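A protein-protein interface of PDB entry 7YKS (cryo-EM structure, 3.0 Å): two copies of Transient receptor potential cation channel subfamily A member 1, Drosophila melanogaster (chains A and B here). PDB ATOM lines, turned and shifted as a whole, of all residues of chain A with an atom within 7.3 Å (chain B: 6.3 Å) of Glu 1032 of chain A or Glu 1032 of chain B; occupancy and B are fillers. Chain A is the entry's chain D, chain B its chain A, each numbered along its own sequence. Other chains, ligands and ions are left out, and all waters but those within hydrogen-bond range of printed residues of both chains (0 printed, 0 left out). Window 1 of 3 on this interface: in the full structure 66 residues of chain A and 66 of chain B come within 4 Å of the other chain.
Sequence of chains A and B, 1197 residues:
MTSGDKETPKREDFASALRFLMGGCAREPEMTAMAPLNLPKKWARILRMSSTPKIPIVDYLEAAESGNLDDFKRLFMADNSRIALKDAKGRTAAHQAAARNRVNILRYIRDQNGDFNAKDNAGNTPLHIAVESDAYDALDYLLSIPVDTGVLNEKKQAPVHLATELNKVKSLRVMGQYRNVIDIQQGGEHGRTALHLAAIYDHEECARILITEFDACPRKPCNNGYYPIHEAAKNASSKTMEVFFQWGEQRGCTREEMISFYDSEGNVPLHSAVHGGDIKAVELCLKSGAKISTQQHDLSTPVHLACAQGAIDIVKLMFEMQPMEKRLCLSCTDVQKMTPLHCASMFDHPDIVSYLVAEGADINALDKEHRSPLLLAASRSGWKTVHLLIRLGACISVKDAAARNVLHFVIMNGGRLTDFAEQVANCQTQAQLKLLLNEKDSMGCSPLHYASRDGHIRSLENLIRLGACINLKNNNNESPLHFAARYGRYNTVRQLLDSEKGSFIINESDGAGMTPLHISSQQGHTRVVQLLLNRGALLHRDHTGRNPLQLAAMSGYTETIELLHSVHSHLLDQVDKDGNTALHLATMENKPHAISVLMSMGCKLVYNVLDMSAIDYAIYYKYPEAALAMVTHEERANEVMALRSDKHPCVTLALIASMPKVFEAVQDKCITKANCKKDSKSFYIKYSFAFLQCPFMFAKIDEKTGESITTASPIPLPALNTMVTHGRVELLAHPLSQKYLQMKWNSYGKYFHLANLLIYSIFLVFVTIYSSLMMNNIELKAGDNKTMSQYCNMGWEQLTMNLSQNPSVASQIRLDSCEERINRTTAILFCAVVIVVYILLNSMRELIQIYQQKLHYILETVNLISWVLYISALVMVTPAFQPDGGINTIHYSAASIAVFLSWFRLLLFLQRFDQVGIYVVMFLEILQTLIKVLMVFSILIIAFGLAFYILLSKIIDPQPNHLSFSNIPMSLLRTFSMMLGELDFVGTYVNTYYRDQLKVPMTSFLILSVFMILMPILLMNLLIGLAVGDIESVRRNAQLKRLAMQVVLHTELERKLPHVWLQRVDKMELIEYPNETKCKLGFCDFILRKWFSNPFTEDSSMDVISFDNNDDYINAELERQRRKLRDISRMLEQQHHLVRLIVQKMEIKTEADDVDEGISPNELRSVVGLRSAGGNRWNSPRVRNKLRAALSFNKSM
OD1 of Asp 1030 of chain B lies within salt-bridge range of NH1 of Arg 1035 of chain A (3.6 Å).
Val 1028 of chain A touches Gly 1025 of chain B (CG2 to CA, 3.9 Å).
Val 1028 of chain A touches Val 1028 of chain B (CG1 to CG1, 3.998 Å).
Gly 1025 of chain B touches Ile 1031 of chain A.
Glu 1032 of chain A touches Glu 1032 of chain B (OE1 to OE2, 3.6 Å).
Arg 1035 of chain A touches Gly 1029 of chain B (NH1 to CA, 3.5 Å).
Printed residues of chain A that touch a printed residue of chain B: Val 1028, Ile 1031, Glu 1032 and Arg 1035.
Along chain A the printed residues that touch a printed residue of chain B span positions 1028 to 1035.
NE of Arg 1036 of chain B lies within hydrogen-bond range of O of Glu 1032 of chain B.
The guanidinium group (NE) of Arg 1036 of chain A sits at hydrogen-bond distance from the backbone carbonyl oxygen (O) of Glu 1032 of chain A, at 3.4 Å.
Val 1028 of chain A touches its own counterpart, Val 1028 of chain B.
Glu 1032 of chain A touches its own counterpart, Glu 1032 of chain B.
Arg 1035 of chain A touches Gly 1029 of chain B, but with the chains exchanged Gly 1029 of chain A does not touch Arg 1035 of chain B (15.8 Å).
Arg 1035 of chain A touches Asp 1030 of chain B, but with the chains exchanged Asp 1030 of chain A does not touch Arg 1035 of chain B (18.2 Å).
Positions printed for both chains: 1027, 1028, 1029, 1030, 1031, 1032, 1033, 1034, 1035, 1036 and 1037.
Of the 6 pairs that touch across the chains among the printed residues, 2 have their exchanged pair printed and touching as well.
Glu 1032 of chain A touches just one residue of chain B: Glu 1032.
Of the printed residues of chain B, Arg 1035 of chain A touches Gly 1029 and Asp 1030.
Of the printed residues of chain A, Gly 1025 of chain B touches Val 1028 (3.9 Å) and Ile 1031 (3.7 Å).
Printed residues of chain A within 4 Å of Asp 1030 of chain B: Arg 1035.
Glu 1032 of chain B touches just one residue of chain A: Glu 1032.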
ATOM      1  N   MET A 922      -7.648  -9.860  16.873  1.00  0.00           N
ATOM      2  CA  MET A 922      -7.944  -8.479  17.240  1.00  0.00           C
ATOM      3  C   MET A 922      -7.768  -7.527  16.066  1.00  0.00           C
ATOM      4  O   MET A 922      -8.477  -6.525  15.976  1.00  0.00           O
ATOM      5  CB  MET A 922      -7.046  -8.035  18.389  1.00  0.00           C
ATOM      6  CG  MET A 922      -7.299  -8.728  19.696  1.00  0.00           C
ATOM      7  SD  MET A 922      -6.120  -8.202  20.933  1.00  0.00           S
ATOM      8  CE  MET A 922      -6.570  -9.262  22.288  1.00  0.00           C
ATOM      9  N   ALA A1027     -12.028   0.895  19.021  1.00  0.00           N
ATOM     10  CA  ALA A1027     -10.991  -0.125  19.048  1.00  0.00           C
ATOM     11  C   ALA A1027     -10.637  -0.550  20.460  1.00  0.00           C
ATOM     12  O   ALA A1027     -10.143  -1.658  20.655  1.00  0.00           O
ATOM     13  CB  ALA A1027      -9.741   0.380  18.339  1.00  0.00           C
ATOM     14  N   VAL A1028     -10.854   0.310  21.453  1.00  0.00           N
ATOM     15  CA  VAL A1028     -10.646  -0.089  22.840  1.00  0.00           C
ATOM     16  C   VAL A1028     -11.730  -1.067  23.270  1.00  0.00           C
ATOM     17  O   VAL A1028     -11.467  -2.033  23.992  1.00  0.00           O
ATOM     18  CB  VAL A1028     -10.591   1.160  23.740  1.00  0.00           C
ATOM     19  CG1 VAL A1028     -10.546   0.797  25.195  1.00  0.00           C
ATOM     20  CG2 VAL A1028      -9.382   1.979  23.405  1.00  0.00           C
ATOM     21  N   GLY A1029     -12.954  -0.869  22.782  1.00  0.00           N
ATOM     22  CA  GLY A1029     -14.044  -1.754  23.143  1.00  0.00           C
ATOM     23  C   GLY A1029     -14.025  -3.091  22.440  1.00  0.00           C
ATOM     24  O   GLY A1029     -14.529  -4.077  22.981  1.00  0.00           O
ATOM     25  N   ASP A1030     -13.462  -3.155  21.233  1.00  0.00           N
ATOM     26  CA  ASP A1030     -13.372  -4.428  20.530  1.00  0.00           C
ATOM     27  C   ASP A1030     -12.231  -5.288  21.043  1.00  0.00           C
ATOM     28  O   ASP A1030     -12.298  -6.513  20.939  1.00  0.00           O
ATOM     29  CB  ASP A1030     -13.192  -4.211  19.030  1.00  0.00           C
ATOM     30  CG  ASP A1030     -14.426  -3.651  18.363  1.00  0.00           C
ATOM     31  OD1 ASP A1030     -15.537  -3.892  18.870  1.00  0.00           O
ATOM     32  OD2 ASP A1030     -14.288  -2.979  17.321  1.00  0.00           O
ATOM     33  N   ILE A1031     -11.178  -4.683  21.584  1.00  0.00           N
ATOM     34  CA  ILE A1031     -10.064  -5.467  22.104  1.00  0.00           C
ATOM     35  C   ILE A1031     -10.423  -6.083  23.449  1.00  0.00           C
ATOM     36  O   ILE A1031     -10.102  -7.245  23.715  1.00  0.00           O
ATOM     37  CB  ILE A1031      -8.796  -4.600  22.170  1.00  0.00           C
ATOM     38  CG1 ILE A1031      -8.304  -4.328  20.761  1.00  0.00           C
ATOM     39  CG2 ILE A1031      -7.697  -5.267  22.937  1.00  0.00           C
ATOM     40  CD1 ILE A1031      -7.255  -3.301  20.696  1.00  0.00           C
ATOM     41  N   GLU A1032     -11.145  -5.355  24.295  1.00  0.00           N
ATOM     42  CA  GLU A1032     -11.562  -5.944  25.560  1.00  0.00           C
ATOM     43  C   GLU A1032     -12.759  -6.871  25.414  1.00  0.00           C
ATOM     44  O   GLU A1032     -13.195  -7.448  26.410  1.00  0.00           O
ATOM     45  CB  GLU A1032     -11.879  -4.862  26.592  1.00  0.00           C
ATOM     46  CG  GLU A1032     -13.154  -4.099  26.355  1.00  0.00           C
ATOM     47  CD  GLU A1032     -13.355  -2.996  27.380  1.00  0.00           C
ATOM     48  OE1 GLU A1032     -12.464  -2.811  28.234  1.00  0.00           O
ATOM     49  OE2 GLU A1032     -14.402  -2.318  27.337  1.00  0.00           O
ATOM     50  N   SER A1033     -13.299  -7.023  24.212  1.00  0.00           N
ATOM     51  CA  SER A1033     -14.288  -8.051  23.934  1.00  0.00           C
ATOM     52  C   SER A1033     -13.660  -9.332  23.413  1.00  0.00           C
ATOM     53  O   SER A1033     -14.187 -10.416  23.670  1.00  0.00           O
ATOM     54  CB  SER A1033     -15.309  -7.536  22.925  1.00  0.00           C
ATOM     55  OG  SER A1033     -16.249  -8.538  22.607  1.00  0.00           O
ATOM     56  N   VAL A1034     -12.553  -9.239  22.676  1.00  0.00           N
ATOM     57  CA  VAL A1034     -11.813 -10.436  22.296  1.00  0.00           C
ATOM     58  C   VAL A1034     -11.076 -10.999  23.499  1.00  0.00           C
ATOM     59  O   VAL A1034     -10.970 -12.215  23.670  1.00  0.00           O
ATOM     60  CB  VAL A1034     -10.847 -10.118  21.141  1.00  0.00           C
ATOM     61  CG1 VAL A1034     -10.069 -11.341  20.713  1.00  0.00           C
ATOM     62  CG2 VAL A1034     -11.591  -9.562  19.980  1.00  0.00           C
ATOM     63  N   ARG A1035     -10.590 -10.124  24.373  1.00  0.00           N
ATOM     64  CA  ARG A1035      -9.754 -10.560  25.482  1.00  0.00           C
ATOM     65  C   ARG A1035     -10.564 -11.262  26.569  1.00  0.00           C
ATOM     66  O   ARG A1035     -10.046 -12.169  27.233  1.00  0.00           O
ATOM     67  CB  ARG A1035      -8.993  -9.353  26.027  1.00  0.00           C
ATOM     68  CG  ARG A1035      -8.077  -9.630  27.185  1.00  0.00           C
ATOM     69  CD  ARG A1035      -7.300  -8.404  27.583  1.00  0.00           C
ATOM     70  NE  ARG A1035      -6.173  -8.140  26.698  1.00  0.00           N
ATOM     71  CZ  ARG A1035      -5.465  -7.019  26.724  1.00  0.00           C
ATOM     72  NH1 ARG A1035      -5.783  -6.049  27.562  1.00  0.00           N
ATOM     73  NH2 ARG A1035      -4.443  -6.864  25.909  1.00  0.00           N
ATOM     74  N   ARG A1036     -11.835 -10.894  26.751  1.00  0.00           N
ATOM     75  CA  ARG A1036     -12.693 -11.660  27.651  1.00  0.00           C
ATOM     76  C   ARG A1036     -13.032 -13.022  27.067  1.00  0.00           C
ATOM     77  O   ARG A1036     -13.053 -14.024  27.785  1.00  0.00           O
ATOM     78  CB  ARG A1036     -13.984 -10.907  27.952  1.00  0.00           C
ATOM     79  CG  ARG A1036     -13.853  -9.732  28.880  1.00  0.00           C
ATOM     80  CD  ARG A1036     -15.229  -9.205  29.240  1.00  0.00           C
ATOM     81  NE  ARG A1036     -15.891  -8.556  28.114  1.00  0.00           N
ATOM     82  CZ  ARG A1036     -16.949  -9.052  27.482  1.00  0.00           C
ATOM     83  NH1 ARG A1036     -17.461 -10.217  27.855  1.00  0.00           N
ATOM     84  NH2 ARG A1036     -17.491  -8.389  26.469  1.00  0.00           N
ATOM     85  N   ASN A1037     -13.299 -13.075  25.767  1.00  0.00           N
ATOM     86  CA  ASN A1037     -13.674 -14.302  25.080  1.00  0.00           C
ATOM     87  C   ASN A1037     -12.486 -14.969  24.409  1.00  0.00           C
ATOM     88  O   ASN A1037     -12.637 -15.563  23.341  1.00  0.00           O
ATOM     89  CB  ASN A1037     -14.759 -14.004  24.051  1.00  0.00           C
ATOM     90  CG  ASN A1037     -16.029 -13.514  24.685  1.00  0.00           C
ATOM     91  OD1 ASN A1037     -16.446 -14.013  25.723  1.00  0.00           O
ATOM     92  ND2 ASN A1037     -16.655 -12.528  24.066  1.00  0.00           N
ATOM     93  N   GLY B1025      -5.408   0.306  22.369  1.00  0.00           N
ATOM     94  CA  GLY B1025      -6.403  -0.516  23.029  1.00  0.00           C
ATOM     95  C   GLY B1025      -5.821  -1.657  23.834  1.00  0.00           C
ATOM     96  O   GLY B1025      -6.457  -2.138  24.771  1.00  0.00           O
ATOM     97  N   ALA B1027      -3.004  -1.209  25.508  1.00  0.00           N
ATOM     98  CA  ALA B1027      -2.387  -0.551  26.650  1.00  0.00           C
ATOM     99  C   ALA B1027      -3.412  -0.025  27.636  1.00  0.00           C
ATOM    100  O   ALA B1027      -3.094   0.142  28.811  1.00  0.00           O
ATOM    101  CB  ALA B1027      -1.499   0.593  26.178  1.00  0.00           C
ATOM    102  N   VAL B1028      -4.632   0.264  27.187  1.00  0.00           N
ATOM    103  CA  VAL B1028      -5.689   0.656  28.110  1.00  0.00           C
ATOM    104  C   VAL B1028      -6.131  -0.542  28.937  1.00  0.00           C
ATOM    105  O   VAL B1028      -6.404  -0.423  30.136  1.00  0.00           O
ATOM    106  CB  VAL B1028      -6.854   1.292  27.329  1.00  0.00           C
ATOM    107  CG1 VAL B1028      -8.037   1.561  28.213  1.00  0.00           C
ATOM    108  CG2 VAL B1028      -6.410   2.580  26.706  1.00  0.00           C
ATOM    109  N   GLY B1029      -6.147  -1.728  28.329  1.00  0.00           N
ATOM    110  CA  GLY B1029      -6.558  -2.919  29.046  1.00  0.00           C
ATOM    111  C   GLY B1029      -5.519  -3.467  29.996  1.00  0.00           C
ATOM    112  O   GLY B1029      -5.872  -4.106  30.988  1.00  0.00           O
ATOM    113  N   ASP B1030      -4.235  -3.246  29.714  1.00  0.00           N
ATOM    114  CA  ASP B1030      -3.192  -3.710  30.620  1.00  0.00           C
ATOM    115  C   ASP B1030      -3.026  -2.796  31.820  1.00  0.00           C
ATOM    116  O   ASP B1030      -2.587  -3.252  32.875  1.00  0.00           O
ATOM    117  CB  ASP B1030      -1.853  -3.825  29.897  1.00  0.00           C
ATOM    118  CG  ASP B1030      -1.821  -4.951  28.891  1.00  0.00           C
ATOM    119  OD1 ASP B1030      -2.562  -5.935  29.075  1.00  0.00           O
ATOM    120  OD2 ASP B1030      -1.042  -4.863  27.920  1.00  0.00           O
ATOM    121  N   ILE B1031      -3.353  -1.513  31.688  1.00  0.00           N
ATOM    122  CA  ILE B1031      -3.225  -0.600  32.817  1.00  0.00           C
ATOM    123  C   ILE B1031      -4.362  -0.806  33.807  1.00  0.00           C
ATOM    124  O   ILE B1031      -4.148  -0.799  35.022  1.00  0.00           O
ATOM    125  CB  ILE B1031      -3.135   0.850  32.312  1.00  0.00           C
ATOM    126  CG1 ILE B1031      -1.793   1.061  31.636  1.00  0.00           C
ATOM    127  CG2 ILE B1031      -3.269   1.842  33.425  1.00  0.00           C
ATOM    128  CD1 ILE B1031      -1.706   2.325  30.894  1.00  0.00           C
ATOM    129  N   GLU B1032      -5.574  -1.058  33.320  1.00  0.00           N
ATOM    130  CA  GLU B1032      -6.668  -1.330  34.243  1.00  0.00           C
ATOM    131  C   GLU B1032      -6.644  -2.749  34.786  1.00  0.00           C
ATOM    132  O   GLU B1032      -7.505  -3.096  35.594  1.00  0.00           O
ATOM    133  CB  GLU B1032      -8.021  -1.057  33.589  1.00  0.00           C
ATOM    134  CG  GLU B1032      -8.448  -2.061  32.551  1.00  0.00           C
ATOM    135  CD  GLU B1032      -9.764  -1.676  31.899  1.00  0.00           C
ATOM    136  OE1 GLU B1032     -10.299  -0.598  32.231  1.00  0.00           O
ATOM    137  OE2 GLU B1032     -10.267  -2.449  31.058  1.00  0.00           O
ATOM    138  N   SER B1033      -5.693  -3.573  34.364  1.00  0.00           N
ATOM    139  CA  SER B1033      -5.455  -4.863  34.991  1.00  0.00           C
ATOM    140  C   SER B1033      -4.399  -4.789  36.080  1.00  0.00           C
ATOM    141  O   SER B1033      -4.475  -5.545  37.051  1.00  0.00           O
ATOM    142  CB  SER B1033      -5.033  -5.885  33.940  1.00  0.00           C
ATOM    143  OG  SER B1033      -4.750  -7.130  34.538  1.00  0.00           O
ATOM    144  N   VAL B1034      -3.408  -3.908  35.942  1.00  0.00           N
ATOM    145  CA  VAL B1034      -2.469  -3.674  37.032  1.00  0.00           C
ATOM    146  C   VAL B1034      -3.141  -2.883  38.141  1.00  0.00           C
ATOM    147  O   VAL B1034      -2.895  -3.113  39.326  1.00  0.00           O
ATOM    148  CB  VAL B1034      -1.215  -2.952  36.505  1.00  0.00           C
ATOM    149  CG1 VAL B1034      -0.213  -2.700  37.608  1.00  0.00           C
ATOM    150  CG2 VAL B1034      -0.581  -3.741  35.417  1.00  0.00           C
ATOM    151  N   ARG B1035      -4.032  -1.967  37.775  1.00  0.00           N
ATOM    152  CA  ARG B1035      -4.627  -1.069  38.755  1.00  0.00           C
ATOM    153  C   ARG B1035      -5.653  -1.778  39.635  1.00  0.00           C
ATOM    154  O   ARG B1035      -5.809  -1.419  40.808  1.00  0.00           O
ATOM    155  CB  ARG B1035      -5.233   0.125  38.020  1.00  0.00           C
ATOM    156  CG  ARG B1035      -5.893   1.158  38.890  1.00  0.00           C
ATOM    157  CD  ARG B1035      -6.367   2.338  38.087  1.00  0.00           C
ATOM    158  NE  ARG B1035      -5.289   3.255  37.743  1.00  0.00           N
ATOM    159  CZ  ARG B1035      -5.420   4.255  36.881  1.00  0.00           C
ATOM    160  NH1 ARG B1035      -6.567   4.448  36.254  1.00  0.00           N
ATOM    161  NH2 ARG B1035      -4.406   5.058  36.641  1.00  0.00           N
ATOM    162  N   ARG B1036      -6.337  -2.800  39.114  1.00  0.00           N
ATOM    163  CA  ARG B1036      -7.191  -3.617  39.972  1.00  0.00           C
ATOM    164  C   ARG B1036      -6.367  -4.476  40.916  1.00  0.00           C
ATOM    165  O   ARG B1036      -6.717  -4.632  42.089  1.00  0.00           O
ATOM    166  CB  ARG B1036      -8.104  -4.514  39.144  1.00  0.00           C
ATOM    167  CG  ARG B1036      -9.248  -3.823  38.456  1.00  0.00           C
ATOM    168  CD  ARG B1036     -10.174  -4.853  37.837  1.00  0.00           C
ATOM    169  NE  ARG B1036      -9.572  -5.530  36.693  1.00  0.00           N
ATOM    170  CZ  ARG B1036      -9.197  -6.804  36.692  1.00  0.00           C
ATOM    171  NH1 ARG B1036      -9.347  -7.543  37.783  1.00  0.00           N
ATOM    172  NH2 ARG B1036      -8.662  -7.339  35.603  1.00  0.00           N
ATOM    173  N   ASN B1037      -5.270  -5.041  40.423  1.00  0.00           N
ATOM    174  CA  ASN B1037      -4.407  -5.917  41.200  1.00  0.00           C
ATOM    175  C   ASN B1037      -3.220  -5.175  41.790  1.00  0.00           C
ATOM    176  O   ASN B1037      -2.131  -5.741  41.897  1.00  0.00           O
ATOM    177  CB  ASN B1037      -3.922  -7.068  40.326  1.00  0.00           C
ATOM    178  CG  ASN B1037      -5.048  -7.948  39.865  1.00  0.00           C
ATOM    179  OD1 ASN B1037      -5.965  -8.244  40.622  1.00  0.00           O
ATOM    180  ND2 ASN B1037      -4.992  -8.373  38.614  1.00  0.00           N
